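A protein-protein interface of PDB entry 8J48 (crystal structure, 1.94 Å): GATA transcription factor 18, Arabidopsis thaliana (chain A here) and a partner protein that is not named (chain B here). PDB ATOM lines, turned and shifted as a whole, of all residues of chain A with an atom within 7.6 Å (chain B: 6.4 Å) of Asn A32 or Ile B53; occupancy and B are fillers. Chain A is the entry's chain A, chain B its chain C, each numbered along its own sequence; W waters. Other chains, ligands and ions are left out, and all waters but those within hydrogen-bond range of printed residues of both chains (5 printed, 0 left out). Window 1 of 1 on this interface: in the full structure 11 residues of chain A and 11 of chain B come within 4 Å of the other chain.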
ATOM      1  N   CYS A   9      -4.314  -0.126   3.732  1.00  0.00           N
ATOM      2  CA  CYS A   9      -5.408  -0.814   3.007  1.00  0.00           C
ATOM      3  C   CYS A   9      -5.940  -1.956   3.872  1.00  0.00           C
ATOM      4  O   CYS A   9      -5.129  -2.763   4.348  1.00  0.00           O
ATOM      5  CB  CYS A   9      -4.938  -1.360   1.669  1.00  0.00           C
ATOM      6  SG  CYS A   9      -6.224  -2.301   0.809  1.00  0.00           S
ATOM      7  N   CYS A  12      -4.911  -5.243   1.596  1.00  0.00           N
ATOM      8  CA  CYS A  12      -3.505  -5.657   1.298  1.00  0.00           C
ATOM      9  C   CYS A  12      -2.495  -5.040   2.270  1.00  0.00           C
ATOM     10  O   CYS A  12      -1.296  -5.344   2.117  1.00  0.00           O
ATOM     11  CB  CYS A  12      -3.124  -5.387  -0.153  1.00  0.00           C
ATOM     12  SG  CYS A  12      -3.128  -3.634  -0.594  1.00  0.00           S
ATOM     13  N   THR A  14      -1.232  -2.165   2.377  1.00  0.00           N
ATOM     14  CA  THR A  14      -0.195  -1.293   1.769  1.00  0.00           C
ATOM     15  C   THR A  14      -0.350   0.132   2.298  1.00  0.00           C
ATOM     16  O   THR A  14      -1.477   0.504   2.679  1.00  0.00           O
ATOM     17  CB  THR A  14      -0.193  -1.331   0.235  1.00  0.00           C
ATOM     18  OG1 THR A  14       1.077  -0.846  -0.201  1.00  0.00           O
ATOM     19  CG2 THR A  14      -1.280  -0.484  -0.388  1.00  0.00           C
ATOM     20  N   SER A  16       0.902   2.649   0.369  1.00  0.00           N
ATOM     21  CA  SER A  16       1.252   3.388  -0.835  1.00  0.00           C
ATOM     22  C   SER A  16       0.200   3.116  -1.899  1.00  0.00           C
ATOM     23  O   SER A  16       0.051   1.974  -2.350  1.00  0.00           O
ATOM     24  CB  SER A  16       2.640   2.958  -1.318  1.00  0.00           C
ATOM     25  OG  SER A  16       3.163   3.841  -2.285  1.00  0.00           O
ATOM     26  N   THR A  17      -0.518   4.166  -2.302  1.00  0.00           N
ATOM     27  CA  THR A  17      -1.543   4.089  -3.333  1.00  0.00           C
ATOM     28  C   THR A  17      -1.754   5.485  -3.910  1.00  0.00           C
ATOM     29  O   THR A  17      -1.529   6.478  -3.208  1.00  0.00           O
ATOM     30  CB  THR A  17      -2.858   3.538  -2.763  1.00  0.00           C
ATOM     31  OG1 THR A  17      -3.723   3.138  -3.830  1.00  0.00           O
ATOM     32  CG2 THR A  17      -3.569   4.589  -1.945  1.00  0.00           C
ATOM     33  N   PRO A  18      -2.174   5.600  -5.176  1.00  0.00           N
ATOM     34  CA  PRO A  18      -2.529   6.921  -5.713  1.00  0.00           C
ATOM     35  C   PRO A  18      -3.907   7.409  -5.301  1.00  0.00           C
ATOM     36  O   PRO A  18      -4.204   8.598  -5.475  1.00  0.00           O
ATOM     37  CB  PRO A  18      -2.461   6.703  -7.234  1.00  0.00           C
ATOM     38  CG  PRO A  18      -2.823   5.273  -7.412  1.00  0.00           C
ATOM     39  CD  PRO A  18      -2.161   4.567  -6.233  1.00  0.00           C
ATOM     40  N   LEU A  19      -4.769   6.537  -4.792  1.00  0.00           N
ATOM     41  CA  LEU A  19      -6.126   6.956  -4.463  1.00  0.00           C
ATOM     42  C   LEU A  19      -6.678   5.976  -3.447  1.00  0.00           C
ATOM     43  O   LEU A  19      -6.595   4.763  -3.655  1.00  0.00           O
ATOM     44  CB  LEU A  19      -7.013   7.000  -5.710  1.00  0.00           C
ATOM     45  CG  LEU A  19      -8.491   7.317  -5.484  1.00  0.00           C
ATOM     46  CD1 LEU A  19      -8.634   8.763  -5.064  1.00  0.00           C
ATOM     47  CD2 LEU A  19      -9.313   7.027  -6.729  1.00  0.00           C
ATOM     48  N   TRP A  20      -7.197   6.492  -2.339  1.00  0.00           N
ATOM     49  CA  TRP A  20      -7.840   5.646  -1.341  1.00  0.00           C
ATOM     50  C   TRP A  20      -9.306   5.508  -1.723  1.00  0.00           C
ATOM     51  O   TRP A  20      -9.956   6.502  -2.066  1.00  0.00           O
ATOM     52  CB  TRP A  20      -7.672   6.226   0.067  1.00  0.00           C
ATOM     53  CG  TRP A  20      -6.258   6.100   0.561  1.00  0.00           C
ATOM     54  CD1 TRP A  20      -5.322   7.089   0.631  1.00  0.00           C
ATOM     55  CD2 TRP A  20      -5.609   4.900   1.011  1.00  0.00           C
ATOM     56  NE1 TRP A  20      -4.134   6.580   1.107  1.00  0.00           N
ATOM     57  CE2 TRP A  20      -4.286   5.241   1.351  1.00  0.00           C
ATOM     58  CE3 TRP A  20      -6.022   3.572   1.164  1.00  0.00           C
ATOM     59  CZ2 TRP A  20      -3.368   4.301   1.831  1.00  0.00           C
ATOM     60  CZ3 TRP A  20      -5.118   2.645   1.650  1.00  0.00           C
ATOM     61  CH2 TRP A  20      -3.805   3.013   1.977  1.00  0.00           C
ATOM     62  N   ARG A  21      -9.808   4.273  -1.718  1.00  0.00           N
ATOM     63  CA  ARG A  21     -11.104   3.966  -2.303  1.00  0.00           C
ATOM     64  C   ARG A  21     -12.035   3.327  -1.281  1.00  0.00           C
ATOM     65  O   ARG A  21     -11.607   2.807  -0.250  1.00  0.00           O
ATOM     66  CB  ARG A  21     -10.962   3.031  -3.513  1.00  0.00           C
ATOM     67  CG  ARG A  21     -10.232   3.649  -4.712  1.00  0.00           C
ATOM     68  CD  ARG A  21     -10.311   2.710  -5.908  1.00  0.00           C
ATOM     69  NE  ARG A  21      -9.910   3.365  -7.153  1.00  0.00           N
ATOM     70  CZ  ARG A  21     -10.741   4.015  -7.964  1.00  0.00           C
ATOM     71  NH1 ARG A  21     -12.035   4.100  -7.679  1.00  0.00           N
ATOM     72  NH2 ARG A  21     -10.271   4.575  -9.070  1.00  0.00           N
ATOM     73  N   LEU A  30      -9.749   1.114   1.288  1.00  0.00           N
ATOM     74  CA  LEU A  30      -8.964   0.235   0.432  1.00  0.00           C
ATOM     75  C   LEU A  30      -8.021   1.063  -0.436  1.00  0.00           C
ATOM     76  O   LEU A  30      -8.316   2.210  -0.783  1.00  0.00           O
ATOM     77  CB  LEU A  30      -9.860  -0.624  -0.474  1.00  0.00           C
ATOM     78  CG  LEU A  30     -10.870  -1.598   0.140  1.00  0.00           C
ATOM     79  CD1 LEU A  30     -11.635  -2.260  -0.991  1.00  0.00           C
ATOM     80  CD2 LEU A  30     -10.165  -2.626   0.996  1.00  0.00           C
ATOM     81  N   CYS A  31      -6.894   0.459  -0.812  1.00  0.00           N
ATOM     82  CA  CYS A  31      -5.986   1.099  -1.756  1.00  0.00           C
ATOM     83  C   CYS A  31      -6.673   1.185  -3.114  1.00  0.00           C
ATOM     84  O   CYS A  31      -7.819   0.735  -3.275  1.00  0.00           O
ATOM     85  CB  CYS A  31      -4.662   0.333  -1.838  1.00  0.00           C
ATOM     86  SG  CYS A  31      -4.760  -1.265  -2.646  1.00  0.00           S
ATOM     87  N   ASN A  32      -5.998   1.780  -4.096  1.00  0.00           N
ATOM     88  CA  ASN A  32      -6.624   1.962  -5.397  1.00  0.00           C
ATOM     89  C   ASN A  32      -6.887   0.627  -6.084  1.00  0.00           C
ATOM     90  O   ASN A  32      -7.971   0.410  -6.632  1.00  0.00           O
ATOM     91  CB  ASN A  32      -5.760   2.855  -6.278  1.00  0.00           C
ATOM     92  CG  ASN A  32      -6.285   2.935  -7.674  1.00  0.00           C
ATOM     93  OD1 ASN A  32      -7.371   3.451  -7.904  1.00  0.00           O
ATOM     94  ND2 ASN A  32      -5.540   2.384  -8.617  1.00  0.00           N
ATOM     95  N   ALA A  33      -5.905  -0.277  -6.078  1.00  0.00           N
ATOM     96  CA  ALA A  33      -6.085  -1.571  -6.731  1.00  0.00           C
ATOM     97  C   ALA A  33      -7.193  -2.391  -6.066  1.00  0.00           C
ATOM     98  O   ALA A  33      -8.083  -2.922  -6.748  1.00  0.00           O
ATOM     99  CB  ALA A  33      -4.766  -2.342  -6.725  1.00  0.00           C
ATOM    100  N   CYS A  34      -7.150  -2.511  -4.729  1.00  0.00           N
ATOM    101  CA  CYS A  34      -8.172  -3.281  -4.011  1.00  0.00           C
ATOM    102  C   CYS A  34      -9.556  -2.660  -4.170  1.00  0.00           C
ATOM    103  O   CYS A  34     -10.553  -3.377  -4.319  1.00  0.00           O
ATOM    104  CB  CYS A  34      -7.803  -3.389  -2.528  1.00  0.00           C
ATOM    105  SG  CYS A  34      -6.353  -4.422  -2.216  1.00  0.00           S
ATOM    106  N   GLY A  35      -9.647  -1.332  -4.131  1.00  0.00           N
ATOM    107  CA  GLY A  35     -10.928  -0.679  -4.319  1.00  0.00           C
ATOM    108  C   GLY A  35     -11.518  -0.931  -5.694  1.00  0.00           C
ATOM    109  O   GLY A  35     -12.742  -1.014  -5.846  1.00  0.00           O
ATOM    110  N   ILE A  36     -10.665  -1.050  -6.715  1.00  0.00           N
ATOM    111  CA  ILE A  36     -11.172  -1.350  -8.055  1.00  0.00           C
ATOM    112  C   ILE A  36     -11.590  -2.815  -8.159  1.00  0.00           C
ATOM    113  O   ILE A  36     -12.611  -3.141  -8.779  1.00  0.00           O
ATOM    114  CB  ILE A  36     -10.126  -0.972  -9.125  1.00  0.00           C
ATOM    115  CG1 ILE A  36      -9.988   0.558  -9.212  1.00  0.00           C
ATOM    116  CG2 ILE A  36     -10.519  -1.568 -10.467  1.00  0.00           C
ATOM    117  CD1 ILE A  36      -8.825   1.068 -10.108  1.00  0.00           C
ATOM    118  N   ARG A  37     -10.810  -3.724  -7.564  1.00  0.00           N
ATOM    119  CA  ARG A  37     -11.246  -5.115  -7.484  1.00  0.00           C
ATOM    120  C   ARG A  37     -12.566  -5.223  -6.737  1.00  0.00           C
ATOM    121  O   ARG A  37     -13.455  -5.984  -7.139  1.00  0.00           O
ATOM    122  CB  ARG A  37     -10.183  -5.976  -6.801  1.00  0.00           C
ATOM    123  CG  ARG A  37      -8.851  -5.931  -7.525  1.00  0.00           C
ATOM    124  CD  ARG A  37      -8.051  -7.223  -7.370  1.00  0.00           C
ATOM    125  NE  ARG A  37      -6.991  -7.266  -8.378  1.00  0.00           N
ATOM    126  CZ  ARG A  37      -5.807  -6.678  -8.234  1.00  0.00           C
ATOM    127  NH1 ARG A  37      -5.532  -6.022  -7.108  1.00  0.00           N
ATOM    128  NH2 ARG A  37      -4.900  -6.748  -9.213  1.00  0.00           N
ATOM    129  N   PHE A  38     -12.719  -4.463  -5.652  1.00  0.00           N
ATOM    130  CA  PHE A  38     -13.957  -4.540  -4.885  1.00  0.00           C
ATOM    131  C   PHE A  38     -15.144  -4.109  -5.733  1.00  0.00           C
ATOM    132  O   PHE A  38     -16.146  -4.829  -5.831  1.00  0.00           O
ATOM    133  CB  PHE A  38     -13.861  -3.689  -3.624  1.00  0.00           C
ATOM    134  CG  PHE A  38     -15.162  -3.596  -2.869  1.00  0.00           C
ATOM    135  CD1 PHE A  38     -15.697  -4.713  -2.249  1.00  0.00           C
ATOM    136  CD2 PHE A  38     -15.852  -2.394  -2.784  1.00  0.00           C
ATOM    137  CE1 PHE A  38     -16.887  -4.635  -1.548  1.00  0.00           C
ATOM    138  CE2 PHE A  38     -17.056  -2.310  -2.087  1.00  0.00           C
ATOM    139  CZ  PHE A  38     -17.566  -3.440  -1.467  1.00  0.00           C
ATOM    140  N   LYS A  40     -15.388  -4.189  -8.881  1.00  0.00           N
ATOM    141  CA  LYS A  40     -15.641  -5.266  -9.837  1.00  0.00           C
ATOM    142  C   LYS A  40     -16.444  -6.387  -9.181  1.00  0.00           C
ATOM    143  O   LYS A  40     -17.379  -6.928  -9.783  1.00  0.00           O
ATOM    144  CB  LYS A  40     -14.308  -5.792 -10.399  1.00  0.00           C
ATOM    145  CG  LYS A  40     -14.387  -6.947 -11.412  1.00  0.00           C
ATOM    146  CD  LYS A  40     -14.048  -8.277 -10.760  1.00  0.00           C
ATOM    147  CE  LYS A  40     -13.447  -9.299 -11.714  1.00  0.00           C
ATOM    148  NZ  LYS A  40     -14.167  -9.432 -13.007  1.00  0.00           N
ATOM    149  N   TYR B  33      -4.099   7.407 -15.274  1.00  0.00           N
ATOM    150  CA  TYR B  33      -4.579   6.036 -15.330  1.00  0.00           C
ATOM    151  C   TYR B  33      -3.551   5.013 -14.894  1.00  0.00           C
ATOM    152  O   TYR B  33      -3.939   3.911 -14.494  1.00  0.00           O
ATOM    153  CB  TYR B  33      -5.045   5.696 -16.752  1.00  0.00           C
ATOM    154  CG  TYR B  33      -6.147   6.613 -17.181  1.00  0.00           C
ATOM    155  CD1 TYR B  33      -7.348   6.627 -16.495  1.00  0.00           C
ATOM    156  CD2 TYR B  33      -5.972   7.509 -18.219  1.00  0.00           C
ATOM    157  CE1 TYR B  33      -8.359   7.475 -16.859  1.00  0.00           C
ATOM    158  CE2 TYR B  33      -6.981   8.355 -18.599  1.00  0.00           C
ATOM    159  CZ  TYR B  33      -8.174   8.340 -17.911  1.00  0.00           C
ATOM    160  OH  TYR B  33      -9.197   9.196 -18.270  1.00  0.00           O
ATOM    161  N   ASP B  35      -1.112   3.238 -12.382  1.00  0.00           N
ATOM    162  CA  ASP B  35      -0.892   3.051 -10.943  1.00  0.00           C
ATOM    163  C   ASP B  35       0.576   2.682 -10.757  1.00  0.00           C
ATOM    164  O   ASP B  35       0.973   1.536 -10.981  1.00  0.00           O
ATOM    165  CB  ASP B  35      -1.811   1.976 -10.362  1.00  0.00           C
ATOM    166  CG  ASP B  35      -1.825   1.979  -8.820  1.00  0.00           C
ATOM    167  OD1 ASP B  35      -0.749   2.179  -8.206  1.00  0.00           O
ATOM    168  OD2 ASP B  35      -2.912   1.772  -8.222  1.00  0.00           O
ATOM    169  N   THR B  37       2.322   2.376  -8.087  1.00  0.00           N
ATOM    170  CA  THR B  37       2.665   1.621  -6.889  1.00  0.00           C
ATOM    171  C   THR B  37       2.643   0.119  -7.107  1.00  0.00           C
ATOM    172  O   THR B  37       2.923  -0.625  -6.166  1.00  0.00           O
ATOM    173  CB  THR B  37       1.705   1.976  -5.747  1.00  0.00           C
ATOM    174  OG1 THR B  37       0.428   1.374  -5.993  1.00  0.00           O
ATOM    175  CG2 THR B  37       1.538   3.490  -5.642  1.00  0.00           C
ATOM    176  N   LEU B  38       2.325  -0.348  -8.311  1.00  0.00           N
ATOM    177  CA  LEU B  38       2.071  -1.756  -8.554  1.00  0.00           C
ATOM    178  C   LEU B  38       3.266  -2.436  -9.214  1.00  0.00           C
ATOM    179  O   LEU B  38       4.004  -1.836 -10.006  1.00  0.00           O
ATOM    180  CB  LEU B  38       0.836  -1.939  -9.436  1.00  0.00           C
ATOM    181  CG  LEU B  38      -0.496  -1.361  -8.936  1.00  0.00           C
ATOM    182  CD1 LEU B  38      -1.601  -1.720  -9.905  1.00  0.00           C
ATOM    183  CD2 LEU B  38      -0.842  -1.840  -7.519  1.00  0.00           C
ATOM    184  N   ARG B  42       0.145  -3.861 -15.979  1.00  0.00           N
ATOM    185  CA  ARG B  42      -1.291  -3.923 -15.786  1.00  0.00           C
ATOM    186  C   ARG B  42      -2.021  -3.329 -16.991  1.00  0.00           C
ATOM    187  O   ARG B  42      -1.456  -2.561 -17.781  1.00  0.00           O
ATOM    188  CB  ARG B  42      -1.712  -3.148 -14.523  1.00  0.00           C
ATOM    189  CG  ARG B  42      -0.814  -3.370 -13.316  1.00  0.00           C
ATOM    190  CD  ARG B  42      -0.928  -4.808 -12.846  1.00  0.00           C
ATOM    191  NE  ARG B  42      -0.048  -5.102 -11.718  1.00  0.00           N
ATOM    192  CZ  ARG B  42      -0.477  -5.315 -10.473  1.00  0.00           C
ATOM    193  NH1 ARG B  42      -1.783  -5.251 -10.184  1.00  0.00           N
ATOM    194  NH2 ARG B  42       0.401  -5.592  -9.511  1.00  0.00           N
ATOM    195  N   TYR B  43      -3.295  -3.699 -17.119  1.00  0.00           N
ATOM    196  CA  TYR B  43      -4.200  -3.094 -18.092  1.00  0.00           C
ATOM    197  C   TYR B  43      -5.470  -2.640 -17.378  1.00  0.00           C
ATOM    198  O   TYR B  43      -5.757  -3.066 -16.259  1.00  0.00           O
ATOM    199  CB  TYR B  43      -4.530  -4.068 -19.229  1.00  0.00           C
ATOM    200  CG  TYR B  43      -5.549  -5.150 -18.889  1.00  0.00           C
ATOM    201  CD1 TYR B  43      -5.164  -6.352 -18.305  1.00  0.00           C
ATOM    202  CD2 TYR B  43      -6.901  -4.967 -19.167  1.00  0.00           C
ATOM    203  CE1 TYR B  43      -6.113  -7.357 -17.995  1.00  0.00           C
ATOM    204  CE2 TYR B  43      -7.855  -5.957 -18.843  1.00  0.00           C
ATOM    205  CZ  TYR B  43      -7.452  -7.147 -18.269  1.00  0.00           C
ATOM    206  OH  TYR B  43      -8.404  -8.110 -17.999  1.00  0.00           O
ATOM    207  N   ASN B  44      -6.232  -1.758 -18.025  1.00  0.00           N
ATOM    208  CA  ASN B  44      -7.501  -1.284 -17.478  1.00  0.00           C
ATOM    209  C   ASN B  44      -8.670  -1.974 -18.162  1.00  0.00           C
ATOM    210  O   ASN B  44      -8.662  -2.185 -19.376  1.00  0.00           O
ATOM    211  CB  ASN B  44      -7.665   0.231 -17.632  1.00  0.00           C
ATOM    212  CG  ASN B  44      -7.596   0.668 -19.054  1.00  0.00           C
ATOM    213  OD1 ASN B  44      -6.694   0.260 -19.790  1.00  0.00           O
ATOM    214  ND2 ASN B  44      -8.548   1.510 -19.468  1.00  0.00           N
ATOM    215  N   GLY B  45      -9.683  -2.306 -17.373  1.00  0.00           N
ATOM    216  CA  GLY B  45     -10.893  -2.885 -17.914  1.00  0.00           C
ATOM    217  C   GLY B  45     -11.973  -1.880 -18.202  1.00  0.00           C
ATOM    218  O   GLY B  45     -13.027  -2.249 -18.722  1.00  0.00           O
ATOM    219  N   GLN B  49     -10.181   6.461 -12.536  1.00  0.00           N
ATOM    220  CA  GLN B  49      -8.927   6.977 -11.997  1.00  0.00           C
ATOM    221  C   GLN B  49      -7.965   5.840 -11.674  1.00  0.00           C
ATOM    222  O   GLN B  49      -8.292   4.932 -10.901  1.00  0.00           O
ATOM    223  CB  GLN B  49      -9.204   7.812 -10.746  1.00  0.00           C
ATOM    224  CG  GLN B  49      -9.878   9.139 -11.048  1.00  0.00           C
ATOM    225  CD  GLN B  49      -9.790  10.109  -9.883  1.00  0.00           C
ATOM    226  OE1 GLN B  49     -10.730  10.232  -9.096  1.00  0.00           O
ATOM    227  NE2 GLN B  49      -8.657  10.808  -9.769  1.00  0.00           N
ATOM    228  N   PHE B  50      -6.779   5.896 -12.263  1.00  0.00           N
ATOM    229  CA  PHE B  50      -5.725   4.929 -11.999  1.00  0.00           C
ATOM    230  C   PHE B  50      -6.220   3.494 -12.207  1.00  0.00           C
ATOM    231  O   PHE B  50      -5.950   2.592 -11.418  1.00  0.00           O
ATOM    232  CB  PHE B  50      -5.157   5.132 -10.594  1.00  0.00           C
ATOM    233  CG  PHE B  50      -4.885   6.566 -10.261  1.00  0.00           C
ATOM    234  CD1 PHE B  50      -3.869   7.260 -10.894  1.00  0.00           C
ATOM    235  CD2 PHE B  50      -5.648   7.225  -9.314  1.00  0.00           C
ATOM    236  CE1 PHE B  50      -3.632   8.593 -10.591  1.00  0.00           C
ATOM    237  CE2 PHE B  50      -5.402   8.549  -9.001  1.00  0.00           C
ATOM    238  CZ  PHE B  50      -4.404   9.233  -9.635  1.00  0.00           C
ATOM    239  N   ALA B  51      -6.918   3.277 -13.316  1.00  0.00           N
ATOM    240  CA  ALA B  51      -7.625   2.024 -13.547  1.00  0.00           C
ATOM    241  C   ALA B  51      -6.740   0.890 -14.067  1.00  0.00           C
ATOM    242  O   ALA B  51      -7.218  -0.246 -14.179  1.00  0.00           O
ATOM    243  CB  ALA B  51      -8.762   2.262 -14.542  1.00  0.00           C
ATOM    244  N   MET B  52      -5.491   1.160 -14.433  1.00  0.00           N
ATOM    245  CA  MET B  52      -4.611   0.107 -14.946  1.00  0.00           C
ATOM    246  C   MET B  52      -4.109  -0.732 -13.772  1.00  0.00           C
ATOM    247  O   MET B  52      -3.020  -0.517 -13.235  1.00  0.00           O
ATOM    248  CB  MET B  52      -3.450   0.714 -15.730  1.00  0.00           C
ATOM    249  CG  MET B  52      -3.853   1.453 -16.994  1.00  0.00           C
ATOM    250  SD  MET B  52      -2.432   2.348 -17.683  1.00  0.00           S
ATOM    251  CE  MET B  52      -1.267   1.015 -17.907  1.00  0.00           C
ATOM    252  N   ILE B  53      -4.926  -1.704 -13.342  1.00  0.00           N
ATOM    253  CA  ILE B  53      -4.529  -2.498 -12.172  1.00  0.00           C
ATOM    254  C   ILE B  53      -4.586  -4.001 -12.397  1.00  0.00           C
ATOM    255  O   ILE B  53      -4.058  -4.761 -11.581  1.00  0.00           O
ATOM    256  CB  ILE B  53      -5.364  -2.133 -10.932  1.00  0.00           C
ATOM    257  CG1 ILE B  53      -6.837  -2.489 -11.155  1.00  0.00           C
ATOM    258  CG2 ILE B  53      -5.171  -0.665 -10.587  1.00  0.00           C
ATOM    259  CD1 ILE B  53      -7.294  -3.770 -10.399  1.00  0.00           C
ATOM    260  N   TRP B  54      -5.207  -4.452 -13.489  1.00  0.00           N
ATOM    261  CA  TRP B  54      -5.344  -5.886 -13.740  1.00  0.00           C
ATOM    262  C   TRP B  54      -4.072  -6.482 -14.338  1.00  0.00           C
ATOM    263  O   TRP B  54      -3.573  -6.001 -15.362  1.00  0.00           O
ATOM    264  CB  TRP B  54      -6.535  -6.128 -14.660  1.00  0.00           C
ATOM    265  CG  TRP B  54      -7.779  -5.576 -14.038  1.00  0.00           C
ATOM    266  CD1 TRP B  54      -8.422  -4.397 -14.351  1.00  0.00           C
ATOM    267  CD2 TRP B  54      -8.508  -6.160 -12.956  1.00  0.00           C
ATOM    268  NE1 TRP B  54      -9.527  -4.236 -13.532  1.00  0.00           N
ATOM    269  CE2 TRP B  54      -9.593  -5.299 -12.664  1.00  0.00           C
ATOM    270  CE3 TRP B  54      -8.358  -7.340 -12.210  1.00  0.00           C
ATOM    271  CZ2 TRP B  54     -10.538  -5.598 -11.664  1.00  0.00           C
ATOM    272  CZ3 TRP B  54      -9.290  -7.627 -11.203  1.00  0.00           C
ATOM    273  CH2 TRP B  54     -10.365  -6.755 -10.947  1.00  0.00           C
ATOM    274  N   LYS B  55      -3.586  -7.578 -13.742  1.00  0.00           N
ATOM    275  CA  LYS B  55      -2.298  -8.129 -14.161  1.00  0.00           C
ATOM    276  C   LYS B  55      -2.395  -8.784 -15.533  1.00  0.00           C
ATOM    277  O   LYS B  55      -3.220  -9.679 -15.767  1.00  0.00           O
ATOM    278  CB  LYS B  55      -1.763  -9.129 -13.136  1.00  0.00           C
ATOM    279  CG  LYS B  55      -1.575  -8.536 -11.748  1.00  0.00           C
ATOM    280  CD  LYS B  55      -0.958  -9.560 -10.797  1.00  0.00           C
ATOM    281  CE  LYS B  55      -0.949  -9.076  -9.356  1.00  0.00           C
ATOM    282  NZ  LYS B  55      -0.887 -10.239  -8.413  1.00  0.00           N
ATOM    283  N   ASP B  77      -7.193 -10.709 -13.166  1.00  0.00           N
ATOM    284  CA  ASP B  77      -5.754 -10.844 -12.990  1.00  0.00           C
ATOM    285  C   ASP B  77      -5.256 -12.147 -13.594  1.00  0.00           C
ATOM    286  O   ASP B  77      -5.859 -13.206 -13.395  1.00  0.00           O
ATOM    287  CB  ASP B  77      -5.373 -10.811 -11.515  1.00  0.00           C
ATOM    288  CG  ASP B  77      -5.548  -9.442 -10.907  1.00  0.00           C
ATOM    289  OD1 ASP B  77      -5.139  -8.446 -11.551  1.00  0.00           O
ATOM    290  OD2 ASP B  77      -6.092  -9.369  -9.784  1.00  0.00           O
HETATM  291  O   HOH W   1     -12.537   6.549 -10.683  1.00  0.00           O
HETATM  292  O   HOH W   2      -4.806  -9.818  -7.563  1.00  0.00           O
HETATM  293  O   HOH W   3      -3.046   0.737  -5.485  1.00  0.00           O
HETATM  294  O   HOH W   4       0.022  -0.170  -3.919  1.00  0.00           O
HETATM  295  O   HOH W   5      -2.306  -5.554  -7.178  1.00  0.00           O
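O of Ser A16 touches OG1 of Thr B37, at 3.7 Å. CG2 of Thr B37 touches CA of Thr A17 (3.9 Å). Pro A18 touches Asp B35. CG2 of Thr B37 touches CD of Pro A18, at 3.9 Å. Pro A18 touches Phe B50 (O to CE2, 3.7 Å). O of Ala A33 touches CD1 of Ile B53 (3.8 Å). O of Gln B49 touches CD1 of Ile A36 (3.98 Å). Ile A36 touches Ala B51 (CD1 to CA, 3.8 Å). CG2 of Ile A36 touches CG1 of Ile B53, at 3.9 Å. Arg A37 touches Arg B42.
Water W2 lies within hydrogen-bond range of OD2 of Asp B77 (2.6 Å) and NE of Arg A37 (3.5 Å). Water W4 lies within hydrogen-bond range of the side-chain hydroxyl (OG1) of Thr B37 (2.6 Å) and the backbone carbonyl oxygen (O) of Ser A16 (2.7 Å). Water W3 lies within hydrogen-bond range of the side-chain carboxylate (OD2) of Asp B35 (2.9 Å), the side-chain hydroxyl (OG1) of Thr A17 (3.0 Å), the backbone NH (N) of Ala A33 (3.1 Å) and the backbone NH (N) of Asn A32 (3.4 Å). Water W1 lies within hydrogen-bond range of N of Gln B49 (3.0 Å) and NH2 of Arg A21 (3.4 Å). Water W5 lies within hydrogen-bond range of NH1 of Arg B42 (3.1 Å) and NH1 of Arg A37 (3.3 Å).
Of the 16 printed residues of chain B, 9 touch a printed residue of chain A. Printed residues of chain A that touch a printed residue of chain B: Ser A16, Thr A17, Pro A18, Leu A19, Arg A21, Asn A32, Ala A33, Ile A36, Arg A37 and Lys A40. Hydrophobic or aromatic side chains of chain A within 4 Å of the printed part of chain B: Pro A18, Leu A19 and Ile A36.
Asn A32 touches four residues of chain B. Ile B53 touches just these residues of chain A: Asn A32, Ala A33, Ile A36 and Arg A37. Of the printed residues of chain B, Pro A18 touches Asp B35, Thr B37 and Phe B50. Printed residues of chain A within 4 Å of Asp B35: Pro A18 (3.4 Å) and Asn A32 (2.7 Å). Printed residues of chain B within 4 Å of Ile A36: Gln B49, Phe B50, Ala B51 and Ile B53. Of the printed residues of chain A, Ala B51 touches Ile A36 (3.8 Å). Of the printed residues of chain B, Thr A17 touches Thr B37 (3.9 Å). The nearest residue of chain B that does not touch Asn A32 is Ala B51 (5.0 Å). The nearest printed residue of chain B that does not touch Ile A36 is Trp B54 (4.2 Å).
The guanidinium group (NH2) of Arg A37 lies within hydrogen-bond range of the backbone carbonyl oxygen (O) of Ile B53 (3.2 Å). The side-chain amide nitrogen (ND2) of Asn A32 sits at hydrogen-bond distance from the backbone carbonyl oxygen (O) of Phe B50, 2.8 Å away. The side-chain amide oxygen (OD1) of Asn A32 sits close to the backbone carbonyl oxygen (O) of Gln B49 (3.5 Å). The guanidinium group (NH2) of Arg A21 lies within hydrogen-bond range of the backbone carbonyl oxygen (O) of Gln B49 (2.7 Å). NE of Arg A37 is in salt-bridge range of OD2 of Asp B77 (2.7 Å). OD2 of Asp B35 is in hydrogen-bond range of ND2 of Asn A32.
OD1 of Asp B35 lies within hydrogen-bond range of OG1 of Thr B37, 2.6 Å away. The backbone NH of Lys B55 lies within hydrogen-bond range of the side-chain carboxylate of Asp B77 (2.8 Å). The backbone NH of Ala B51 lies within hydrogen-bond range of the backbone carbonyl oxygen of Tyr B33, 3.3 Å away. N of Tyr B43 is in hydrogen-bond range of O of Trp B54, at 2.9 Å. O of Tyr B43 is in hydrogen-bond range of N of Ile B53, 3.3 Å away. The backbone carbonyl oxygen (O) of Leu A30 lies within hydrogen-bond range of the backbone NH (N) of Arg A21 (2.7 Å).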
